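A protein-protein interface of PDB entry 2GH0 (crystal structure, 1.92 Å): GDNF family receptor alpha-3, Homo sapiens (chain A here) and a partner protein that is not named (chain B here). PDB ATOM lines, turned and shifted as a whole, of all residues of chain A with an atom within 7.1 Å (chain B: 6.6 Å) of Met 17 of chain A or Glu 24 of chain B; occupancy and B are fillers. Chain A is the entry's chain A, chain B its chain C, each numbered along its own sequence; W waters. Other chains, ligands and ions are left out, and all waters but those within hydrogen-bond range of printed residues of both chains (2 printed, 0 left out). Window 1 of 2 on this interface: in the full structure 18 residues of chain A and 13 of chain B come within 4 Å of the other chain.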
ATOM      1  N   LEU A  11      17.108  -4.282 -20.867  1.00  0.00           N
ATOM      2  CA  LEU A  11      16.415  -5.354 -20.155  1.00  0.00           C
ATOM      3  C   LEU A  11      15.411  -4.790 -19.161  1.00  0.00           C
ATOM      4  O   LEU A  11      14.446  -5.446 -18.828  1.00  0.00           O
ATOM      5  CB  LEU A  11      17.403  -6.283 -19.414  1.00  0.00           C
ATOM      6  CG  LEU A  11      18.295  -7.060 -20.396  1.00  0.00           C
ATOM      7  CD1 LEU A  11      19.104  -8.113 -19.679  1.00  0.00           C
ATOM      8  CD2 LEU A  11      17.462  -7.720 -21.459  1.00  0.00           C
ATOM      9  N   CYS A  12      15.620  -3.569 -18.688  1.00  0.00           N
ATOM     10  CA  CYS A  12      14.577  -2.975 -17.828  1.00  0.00           C
ATOM     11  C   CYS A  12      13.245  -2.818 -18.600  1.00  0.00           C
ATOM     12  O   CYS A  12      12.196  -3.148 -18.082  1.00  0.00           O
ATOM     13  CB  CYS A  12      15.037  -1.650 -17.252  1.00  0.00           C
ATOM     14  SG  CYS A  12      16.234  -1.996 -15.887  1.00  0.00           S
ATOM     15  N   LEU A  13      13.318  -2.372 -19.849  1.00  0.00           N
ATOM     16  CA  LEU A  13      12.145  -2.281 -20.718  1.00  0.00           C
ATOM     17  C   LEU A  13      11.583  -3.682 -20.948  1.00  0.00           C
ATOM     18  O   LEU A  13      10.385  -3.887 -20.827  1.00  0.00           O
ATOM     19  CB  LEU A  13      12.479  -1.612 -22.076  1.00  0.00           C
ATOM     20  CG  LEU A  13      11.317  -1.517 -23.088  1.00  0.00           C
ATOM     21  CD1 LEU A  13      10.019  -0.941 -22.474  1.00  0.00           C
ATOM     22  CD2 LEU A  13      11.707  -0.711 -24.319  1.00  0.00           C
ATOM     23  N   LYS A  14      12.436  -4.631 -21.334  1.00  0.00           N
ATOM     24  CA  LYS A  14      11.954  -6.014 -21.531  1.00  0.00           C
ATOM     25  C   LYS A  14      11.239  -6.598 -20.302  1.00  0.00           C
ATOM     26  O   LYS A  14      10.160  -7.245 -20.433  1.00  0.00           O
ATOM     27  CB  LYS A  14      13.086  -6.930 -22.016  1.00  0.00           C
ATOM     28  CG  LYS A  14      13.538  -6.628 -23.426  1.00  0.00           C
ATOM     29  CD  LYS A  14      14.699  -7.593 -23.775  1.00  0.00           C
ATOM     30  CE  LYS A  14      15.271  -7.396 -25.177  1.00  0.00           C
ATOM     31  NZ  LYS A  14      15.875  -8.710 -25.707  1.00  0.00           N
ATOM     32  N   PHE A  15      11.810  -6.420 -19.112  1.00  0.00           N
ATOM     33  CA  PHE A  15      11.112  -6.902 -17.906  1.00  0.00           C
ATOM     34  C   PHE A  15       9.800  -6.206 -17.550  1.00  0.00           C
ATOM     35  O   PHE A  15       8.891  -6.840 -17.008  1.00  0.00           O
ATOM     36  CB  PHE A  15      12.036  -6.951 -16.695  1.00  0.00           C
ATOM     37  CG  PHE A  15      12.977  -8.130 -16.737  1.00  0.00           C
ATOM     38  CD1 PHE A  15      14.290  -7.968 -17.188  1.00  0.00           C
ATOM     39  CD2 PHE A  15      12.534  -9.376 -16.328  1.00  0.00           C
ATOM     40  CE1 PHE A  15      15.184  -9.046 -17.263  1.00  0.00           C
ATOM     41  CE2 PHE A  15      13.398 -10.486 -16.408  1.00  0.00           C
ATOM     42  CZ  PHE A  15      14.730 -10.324 -16.875  1.00  0.00           C
ATOM     43  N   ALA A  16       9.717  -4.912 -17.836  1.00  0.00           N
ATOM     44  CA  ALA A  16       8.431  -4.177 -17.736  1.00  0.00           C
ATOM     45  C   ALA A  16       7.439  -4.867 -18.632  1.00  0.00           C
ATOM     46  O   ALA A  16       6.311  -5.115 -18.265  1.00  0.00           O
ATOM     47  CB  ALA A  16       8.596  -2.691 -18.143  1.00  0.00           C
ATOM     48  N   MET A  17       7.856  -5.170 -19.837  1.00  0.00           N
ATOM     49  CA  MET A  17       6.928  -5.795 -20.785  1.00  0.00           C
ATOM     50  C   MET A  17       6.537  -7.254 -20.443  1.00  0.00           C
ATOM     51  O   MET A  17       5.405  -7.687 -20.770  1.00  0.00           O
ATOM     52  CB  MET A  17       7.490  -5.647 -22.199  1.00  0.00           C
ATOM     53  CG  MET A  17       7.535  -4.155 -22.642  1.00  0.00           C
ATOM     54  SD  MET A  17       5.940  -3.286 -22.562  1.00  0.00           S
ATOM     55  CE  MET A  17       5.980  -2.472 -20.987  1.00  0.00           C
ATOM     56  N   LEU A  18       7.443  -8.027 -19.809  1.00  0.00           N
ATOM     57  CA  LEU A  18       7.047  -9.346 -19.263  1.00  0.00           C
ATOM     58  C   LEU A  18       5.919  -9.228 -18.276  1.00  0.00           C
ATOM     59  O   LEU A  18       5.030 -10.064 -18.192  1.00  0.00           O
ATOM     60  CB  LEU A  18       8.196 -10.006 -18.540  1.00  0.00           C
ATOM     61  CG  LEU A  18       9.108 -11.056 -19.077  1.00  0.00           C
ATOM     62  CD1 LEU A  18       9.931 -11.573 -17.849  1.00  0.00           C
ATOM     63  CD2 LEU A  18       8.338 -12.200 -19.805  1.00  0.00           C
ATOM     64  N   CYS A  19       5.934  -8.175 -17.476  1.00  0.00           N
ATOM     65  CA  CYS A  19       4.822  -7.896 -16.550  1.00  0.00           C
ATOM     66  C   CYS A  19       3.533  -7.594 -17.335  1.00  0.00           C
ATOM     67  O   CYS A  19       2.435  -8.112 -17.022  1.00  0.00           O
ATOM     68  CB  CYS A  19       5.228  -6.684 -15.640  1.00  0.00           C
ATOM     69  SG  CYS A  19       3.941  -6.110 -14.410  1.00  0.00           S
ATOM     70  N   THR A  20       3.646  -6.740 -18.356  1.00  0.00           N
ATOM     71  CA  THR A  20       2.484  -6.355 -19.173  1.00  0.00           C
ATOM     72  C   THR A  20       1.884  -7.595 -19.817  1.00  0.00           C
ATOM     73  O   THR A  20       0.642  -7.696 -20.038  1.00  0.00           O
ATOM     74  CB  THR A  20       2.929  -5.350 -20.259  1.00  0.00           C
ATOM     75  OG1 THR A  20       3.466  -4.163 -19.625  1.00  0.00           O
ATOM     76  CG2 THR A  20       1.800  -5.003 -21.191  1.00  0.00           C
ATOM     77  N   LEU A  21       2.750  -8.554 -20.151  1.00  0.00           N
ATOM     78  CA  LEU A  21       2.296  -9.816 -20.762  1.00  0.00           C
ATOM     79  C   LEU A  21       1.520 -10.748 -19.796  1.00  0.00           C
ATOM     80  O   LEU A  21       0.852 -11.689 -20.220  1.00  0.00           O
ATOM     81  CB  LEU A  21       3.495 -10.562 -21.363  1.00  0.00           C
ATOM     82  CG  LEU A  21       4.021  -9.988 -22.681  1.00  0.00           C
ATOM     83  CD1 LEU A  21       5.305 -10.766 -22.970  1.00  0.00           C
ATOM     84  CD2 LEU A  21       3.054 -10.180 -23.791  1.00  0.00           C
ATOM     85  N   ASN A  22       1.608 -10.479 -18.502  1.00  0.00           N
ATOM     86  CA  ASN A  22       0.955 -11.326 -17.498  1.00  0.00           C
ATOM     87  C   ASN A  22      -0.242 -10.532 -17.032  1.00  0.00           C
ATOM     88  O   ASN A  22      -0.064  -9.414 -16.582  1.00  0.00           O
ATOM     89  CB  ASN A  22       1.921 -11.615 -16.311  1.00  0.00           C
ATOM     90  CG  ASN A  22       1.243 -12.386 -15.185  1.00  0.00           C
ATOM     91  OD1 ASN A  22       0.766 -11.775 -14.227  1.00  0.00           O
ATOM     92  ND2 ASN A  22       1.106 -13.744 -15.338  1.00  0.00           N
ATOM     93  N   ARG A  29       0.458  -3.143 -12.171  1.00  0.00           N
ATOM     94  CA  ARG A  29       1.451  -2.125 -12.602  1.00  0.00           C
ATOM     95  C   ARG A  29       0.694  -0.924 -13.148  1.00  0.00           C
ATOM     96  O   ARG A  29       1.027   0.214 -12.839  1.00  0.00           O
ATOM     97  CB  ARG A  29       2.365  -2.691 -13.705  1.00  0.00           C
ATOM     98  CG  ARG A  29       3.381  -1.653 -14.217  1.00  0.00           C
ATOM     99  CD  ARG A  29       4.445  -2.334 -15.144  1.00  0.00           C
ATOM    100  NE  ARG A  29       5.247  -1.333 -15.854  1.00  0.00           N
ATOM    101  CZ  ARG A  29       4.929  -0.796 -17.032  1.00  0.00           C
ATOM    102  NH1 ARG A  29       3.839  -1.156 -17.698  1.00  0.00           N
ATOM    103  NH2 ARG A  29       5.744   0.093 -17.574  1.00  0.00           N
ATOM    104  N   LEU A  65      10.778  -6.598 -12.656  1.00  0.00           N
ATOM    105  CA  LEU A  65      10.387  -5.229 -12.985  1.00  0.00           C
ATOM    106  C   LEU A  65      11.417  -4.230 -12.365  1.00  0.00           C
ATOM    107  O   LEU A  65      11.903  -3.250 -12.982  1.00  0.00           O
ATOM    108  CB  LEU A  65       8.991  -4.975 -12.385  1.00  0.00           C
ATOM    109  CG  LEU A  65       8.478  -3.552 -12.670  1.00  0.00           C
ATOM    110  CD1 LEU A  65       8.276  -3.321 -14.175  1.00  0.00           C
ATOM    111  CD2 LEU A  65       7.216  -3.151 -11.867  1.00  0.00           C
ATOM    112  N   ARG A  80      15.304   4.508 -16.356  1.00  0.00           N
ATOM    113  CA  ARG A  80      14.047   3.722 -16.274  1.00  0.00           C
ATOM    114  C   ARG A  80      13.968   2.986 -14.940  1.00  0.00           C
ATOM    115  O   ARG A  80      12.986   3.115 -14.210  1.00  0.00           O
ATOM    116  CB  ARG A  80      13.959   2.721 -17.420  1.00  0.00           C
ATOM    117  CG  ARG A  80      12.855   1.720 -17.192  1.00  0.00           C
ATOM    118  CD  ARG A  80      12.639   0.855 -18.392  1.00  0.00           C
ATOM    119  NE  ARG A  80      11.261   0.518 -18.198  1.00  0.00           N
ATOM    120  CZ  ARG A  80      10.237   1.041 -18.844  1.00  0.00           C
ATOM    121  NH1 ARG A  80      10.370   1.852 -19.906  1.00  0.00           N
ATOM    122  NH2 ARG A  80       9.068   0.637 -18.458  1.00  0.00           N
ATOM    123  N   LEU B  10      -2.225  -6.202 -27.645  1.00  0.00           N
ATOM    124  CA  LEU B  10      -0.992  -5.545 -27.187  1.00  0.00           C
ATOM    125  C   LEU B  10      -0.488  -4.718 -28.376  1.00  0.00           C
ATOM    126  O   LEU B  10      -0.251  -5.269 -29.473  1.00  0.00           O
ATOM    127  CB  LEU B  10       0.055  -6.625 -26.866  1.00  0.00           C
ATOM    128  CG  LEU B  10       1.150  -6.062 -25.979  1.00  0.00           C
ATOM    129  CD1 LEU B  10       0.580  -5.830 -24.601  1.00  0.00           C
ATOM    130  CD2 LEU B  10       2.337  -7.003 -25.960  1.00  0.00           C
ATOM    131  N   VAL B  11      -0.356  -3.417 -28.175  1.00  0.00           N
ATOM    132  CA  VAL B  11       0.048  -2.508 -29.256  1.00  0.00           C
ATOM    133  C   VAL B  11       1.181  -1.561 -28.791  1.00  0.00           C
ATOM    134  O   VAL B  11       1.277  -1.264 -27.589  1.00  0.00           O
ATOM    135  CB  VAL B  11      -1.177  -1.660 -29.750  1.00  0.00           C
ATOM    136  CG1 VAL B  11      -2.301  -2.569 -30.246  1.00  0.00           C
ATOM    137  CG2 VAL B  11      -1.717  -0.709 -28.642  1.00  0.00           C
ATOM    138  N   PRO B  12       2.012  -1.083 -29.729  1.00  0.00           N
ATOM    139  CA  PRO B  12       3.037  -0.105 -29.402  1.00  0.00           C
ATOM    140  C   PRO B  12       2.351   1.187 -28.970  1.00  0.00           C
ATOM    141  O   PRO B  12       1.413   1.621 -29.644  1.00  0.00           O
ATOM    142  CB  PRO B  12       3.724   0.135 -30.742  1.00  0.00           C
ATOM    143  CG  PRO B  12       3.359  -0.989 -31.618  1.00  0.00           C
ATOM    144  CD  PRO B  12       2.032  -1.456 -31.161  1.00  0.00           C
ATOM    145  N   VAL B  13       2.776   1.789 -27.854  1.00  0.00           N
ATOM    146  CA  VAL B  13       2.261   3.126 -27.455  1.00  0.00           C
ATOM    147  C   VAL B  13       2.425   4.114 -28.630  1.00  0.00           C
ATOM    148  O   VAL B  13       1.587   5.009 -28.837  1.00  0.00           O
ATOM    149  CB  VAL B  13       2.948   3.676 -26.171  1.00  0.00           C
ATOM    150  CG1 VAL B  13       2.555   5.135 -25.922  1.00  0.00           C
ATOM    151  CG2 VAL B  13       2.576   2.843 -24.952  1.00  0.00           C
ATOM    152  N   ARG B  14       3.489   3.923 -29.413  1.00  0.00           N
ATOM    153  CA  ARG B  14       3.782   4.741 -30.591  1.00  0.00           C
ATOM    154  C   ARG B  14       2.698   4.729 -31.682  1.00  0.00           C
ATOM    155  O   ARG B  14       2.703   5.599 -32.547  1.00  0.00           O
ATOM    156  CB  ARG B  14       5.149   4.387 -31.209  1.00  0.00           C
ATOM    157  CG  ARG B  14       6.274   5.110 -30.507  1.00  0.00           C
ATOM    158  CD  ARG B  14       7.664   4.617 -30.885  1.00  0.00           C
ATOM    159  NE  ARG B  14       8.702   5.428 -30.236  1.00  0.00           N
ATOM    160  CZ  ARG B  14       9.911   4.973 -29.905  1.00  0.00           C
ATOM    161  NH1 ARG B  14      10.227   3.693 -30.137  1.00  0.00           N
ATOM    162  NH2 ARG B  14      10.808   5.783 -29.322  1.00  0.00           N
ATOM    163  N   SER B  22       6.905   6.886 -26.289  1.00  0.00           N
ATOM    164  CA  SER B  22       7.212   5.774 -25.391  1.00  0.00           C
ATOM    165  C   SER B  22       7.743   4.583 -26.178  1.00  0.00           C
ATOM    166  O   SER B  22       7.416   4.431 -27.356  1.00  0.00           O
ATOM    167  CB  SER B  22       5.972   5.340 -24.605  1.00  0.00           C
ATOM    168  OG  SER B  22       6.325   4.232 -23.789  1.00  0.00           O
ATOM    169  N   ASP B  23       8.571   3.759 -25.548  1.00  0.00           N
ATOM    170  CA  ASP B  23       9.039   2.524 -26.178  1.00  0.00           C
ATOM    171  C   ASP B  23       8.213   1.324 -25.718  1.00  0.00           C
ATOM    172  O   ASP B  23       8.413   0.195 -26.212  1.00  0.00           O
ATOM    173  CB  ASP B  23      10.515   2.288 -25.904  1.00  0.00           C
ATOM    174  CG  ASP B  23      11.421   3.313 -26.588  1.00  0.00           C
ATOM    175  OD1 ASP B  23      12.477   3.661 -26.029  1.00  0.00           O
ATOM    176  OD2 ASP B  23      11.048   3.795 -27.664  1.00  0.00           O
ATOM    177  N   GLU B  24       7.248   1.578 -24.832  1.00  0.00           N
ATOM    178  CA  GLU B  24       6.420   0.513 -24.281  1.00  0.00           C
ATOM    179  C   GLU B  24       5.306  -0.013 -25.202  1.00  0.00           C
ATOM    180  O   GLU B  24       4.906   0.644 -26.195  1.00  0.00           O
ATOM    181  CB  GLU B  24       5.830   0.925 -22.931  1.00  0.00           C
ATOM    182  CG  GLU B  24       6.944   1.246 -21.898  1.00  0.00           C
ATOM    183  CD  GLU B  24       6.414   1.457 -20.469  1.00  0.00           C
ATOM    184  OE1 GLU B  24       5.212   1.357 -20.278  1.00  0.00           O
ATOM    185  OE2 GLU B  24       7.227   1.712 -19.556  1.00  0.00           O
ATOM    186  N   LEU B  25       4.820  -1.209 -24.858  1.00  0.00           N
ATOM    187  CA  LEU B  25       3.598  -1.762 -25.435  1.00  0.00           C
ATOM    188  C   LEU B  25       2.570  -1.721 -24.368  1.00  0.00           C
ATOM    189  O   LEU B  25       2.931  -1.802 -23.167  1.00  0.00           O
ATOM    190  CB  LEU B  25       3.812  -3.225 -25.881  1.00  0.00           C
ATOM    191  CG  LEU B  25       5.091  -3.476 -26.701  1.00  0.00           C
ATOM    192  CD1 LEU B  25       5.514  -4.933 -26.585  1.00  0.00           C
ATOM    193  CD2 LEU B  25       4.835  -3.115 -28.134  1.00  0.00           C
ATOM    194  N   VAL B  26       1.309  -1.511 -24.765  1.00  0.00           N
ATOM    195  CA  VAL B  26       0.204  -1.505 -23.801  1.00  0.00           C
ATOM    196  C   VAL B  26      -0.881  -2.417 -24.300  1.00  0.00           C
ATOM    197  O   VAL B  26      -1.008  -2.576 -25.503  1.00  0.00           O
ATOM    198  CB  VAL B  26      -0.408  -0.116 -23.516  1.00  0.00           C
ATOM    199  CG1 VAL B  26       0.572   0.694 -22.657  1.00  0.00           C
ATOM    200  CG2 VAL B  26      -0.762   0.623 -24.791  1.00  0.00           C
ATOM    201  N   SER B  78      -1.604   3.686 -19.029  1.00  0.00           N
ATOM    202  CA  SER B  78      -0.428   4.286 -18.328  1.00  0.00           C
ATOM    203  C   SER B  78       0.800   3.576 -18.810  1.00  0.00           C
ATOM    204  O   SER B  78       0.753   2.362 -19.058  1.00  0.00           O
ATOM    205  CB  SER B  78      -0.496   4.066 -16.833  1.00  0.00           C
ATOM    206  OG  SER B  78      -1.711   4.613 -16.306  1.00  0.00           O
ATOM    207  N   PHE B  79       1.894   4.318 -18.914  1.00  0.00           N
ATOM    208  CA  PHE B  79       3.129   3.828 -19.464  1.00  0.00           C
ATOM    209  C   PHE B  79       4.215   4.795 -19.020  1.00  0.00           C
ATOM    210  O   PHE B  79       3.929   5.888 -18.576  1.00  0.00           O
ATOM    211  CB  PHE B  79       3.068   3.756 -21.011  1.00  0.00           C
ATOM    212  CG  PHE B  79       2.673   5.063 -21.658  1.00  0.00           C
ATOM    213  CD1 PHE B  79       3.626   6.044 -21.934  1.00  0.00           C
ATOM    214  CD2 PHE B  79       1.341   5.318 -21.965  1.00  0.00           C
ATOM    215  CE1 PHE B  79       3.246   7.272 -22.515  1.00  0.00           C
ATOM    216  CE2 PHE B  79       0.953   6.548 -22.536  1.00  0.00           C
ATOM    217  CZ  PHE B  79       1.924   7.516 -22.809  1.00  0.00           C
ATOM    218  N   MET B  80       5.460   4.375 -19.139  1.00  0.00           N
ATOM    219  CA  MET B  80       6.586   5.265 -18.952  1.00  0.00           C
ATOM    220  C   MET B  80       7.039   5.775 -20.323  1.00  0.00           C
ATOM    221  O   MET B  80       7.157   4.988 -21.261  1.00  0.00           O
ATOM    222  CB  MET B  80       7.752   4.571 -18.231  1.00  0.00           C
ATOM    223  CG  MET B  80       7.504   4.242 -16.756  1.00  0.00           C
ATOM    224  SD  MET B  80       8.883   3.355 -15.935  1.00  0.00           S
ATOM    225  CE  MET B  80       9.970   4.658 -15.549  1.00  0.00           C
ATOM    226  N   ASP B  81       7.229   7.095 -20.449  1.00  0.00           N
ATOM    227  CA  ASP B  81       7.670   7.689 -21.744  1.00  0.00           C
ATOM    228  C   ASP B  81       9.170   7.486 -21.981  1.00  0.00           C
ATOM    229  O   ASP B  81       9.856   6.855 -21.146  1.00  0.00           O
ATOM    230  CB  ASP B  81       7.213   9.164 -21.906  1.00  0.00           C
ATOM    231  CG  ASP B  81       7.915  10.127 -20.984  1.00  0.00           C
ATOM    232  OD1 ASP B  81       9.008   9.832 -20.467  1.00  0.00           O
ATOM    233  OD2 ASP B  81       7.394  11.257 -20.824  1.00  0.00           O
ATOM    234  N   TRP B  86       6.454   8.562 -15.865  1.00  0.00           N
ATOM    235  CA  TRP B  86       5.103   7.975 -15.968  1.00  0.00           C
ATOM    236  C   TRP B  86       4.071   8.966 -16.507  1.00  0.00           C
ATOM    237  O   TRP B  86       3.931  10.084 -15.997  1.00  0.00           O
ATOM    238  CB  TRP B  86       4.624   7.509 -14.598  1.00  0.00           C
ATOM    239  CG  TRP B  86       5.169   6.181 -14.190  1.00  0.00           C
ATOM    240  CD1 TRP B  86       6.237   5.923 -13.381  1.00  0.00           C
ATOM    241  CD2 TRP B  86       4.628   4.913 -14.577  1.00  0.00           C
ATOM    242  NE1 TRP B  86       6.390   4.541 -13.247  1.00  0.00           N
ATOM    243  CE2 TRP B  86       5.420   3.907 -13.978  1.00  0.00           C
ATOM    244  CE3 TRP B  86       3.563   4.535 -15.387  1.00  0.00           C
ATOM    245  CZ2 TRP B  86       5.139   2.530 -14.150  1.00  0.00           C
ATOM    246  CZ3 TRP B  86       3.308   3.162 -15.598  1.00  0.00           C
ATOM    247  CH2 TRP B  86       4.107   2.190 -14.963  1.00  0.00           C
HETATM  248  O   HOH W   1       7.665   0.239 -15.531  1.00  0.00           O
HETATM  249  O   HOH W   2       0.811  -0.428 -19.252  1.00  0.00           O
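Water W2 lies within hydrogen-bond range of the backbone carbonyl oxygen of Ser 78 of chain B (2.8 Å) and the guanidinium group of Arg 29 of chain A (3.5 Å). Water W1 lies within hydrogen-bond range of NH2 of Arg 29 of chain A (2.8 Å), NH2 of Arg 80 of chain A (3.3 Å) and SD of Met 80 of chain B (3.4 Å).
Of the 15 printed residues of chain A, 6 touch a printed residue of chain B. Hydrophobic or aromatic side chains of chain A within 4 Å of the printed part of chain B: Leu 13, Met 17 and Leu 21. Of the 15 printed residues of chain B, 6 touch a printed residue of chain A. Printed residues of chain B that touch a printed residue of chain A: Leu 10, Asp 23, Glu 24, Leu 25, Met 80 and Trp 86. Along chain B the printed residues that touch a printed residue of chain A span positions 10 to 86. Among the printed residues, 11 pairs touch across the chains.
CD2 of Leu 13 of chain A touches CB of Asp 23 of chain B, at 3.6 Å. Leu 13 of chain A touches Glu 24 of chain B (CD1 to CG, 3.8 Å). CE of Met 17 of chain A touches CB of Glu 24 of chain B, 3.9 Å away. CD1 of Leu 10 of chain B touches CG2 of Thr 20 of chain A, 3.7 Å away. Thr 20 of chain A touches Leu 25 of chain B (CG2 to O, 3.9 Å). Leu 10 of chain B touches Leu 21 of chain A (CD2 to CD2, 3.9 Å). CZ of Arg 29 of chain A touches CH2 of Trp 86 of chain B (3.7 Å).
The guanidinium group of Arg 29 of chain A is in salt-bridge range of the side-chain carboxylate of Glu 24 of chain B (3.0 Å). OE2 of Glu 24 of chain B is in salt-bridge range of NH1 of Arg 80 of chain A (3.2 Å). The backbone NH (N) of Leu 25 of chain B sits at hydrogen-bond distance from the side-chain sulfur (SD) of Met 17 of chain A, 3.3 Å away. The guanidinium group (NH2) of Arg 80 of chain A sits at hydrogen-bond distance from the side-chain sulfur (SD) of Met 80 of chain B.
Printed residues of chain B within 4 Å of Met 17 of chain A: Glu 24 and Leu 25. Glu 24 of chain B touches just these residues of chain A: Leu 13, Met 17, Arg 29 and Arg 80. Of the printed residues of chain B, Arg 29 of chain A touches Glu 24 (3.0 Å) and Trp 86 (3.7 Å). Of the printed residues of chain A, Met 80 of chain B touches Arg 80 (3.6 Å). The nearest printed residue of chain B that does not touch Leu 13 of chain A is Leu 25 of chain B (5.7 Å).
The backbone NH (N) of Val 13 of chain B lies within hydrogen-bond range of the backbone carbonyl oxygen (O) of Glu 24 of chain B (2.9 Å). The side-chain carboxylate (OD2) of Asp 23 of chain B is in salt-bridge range of the guanidinium group (NH2) of Arg 14 of chain B, 2.6 Å away. OG of Ser 22 of chain B is in hydrogen-bond range of N of Glu 24 of chain B, 3.0 Å away. OG of Ser 22 of chain B sits at hydrogen-bond distance from O of Met 80 of chain B. The side-chain carboxylate (OE2) of Glu 24 of chain B lies close to the backbone NH (N) of Met 80 of chain B. OG1 of Thr 20 of chain A sits at hydrogen-bond distance from O of Ala 16 of chain A (3.3 Å).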
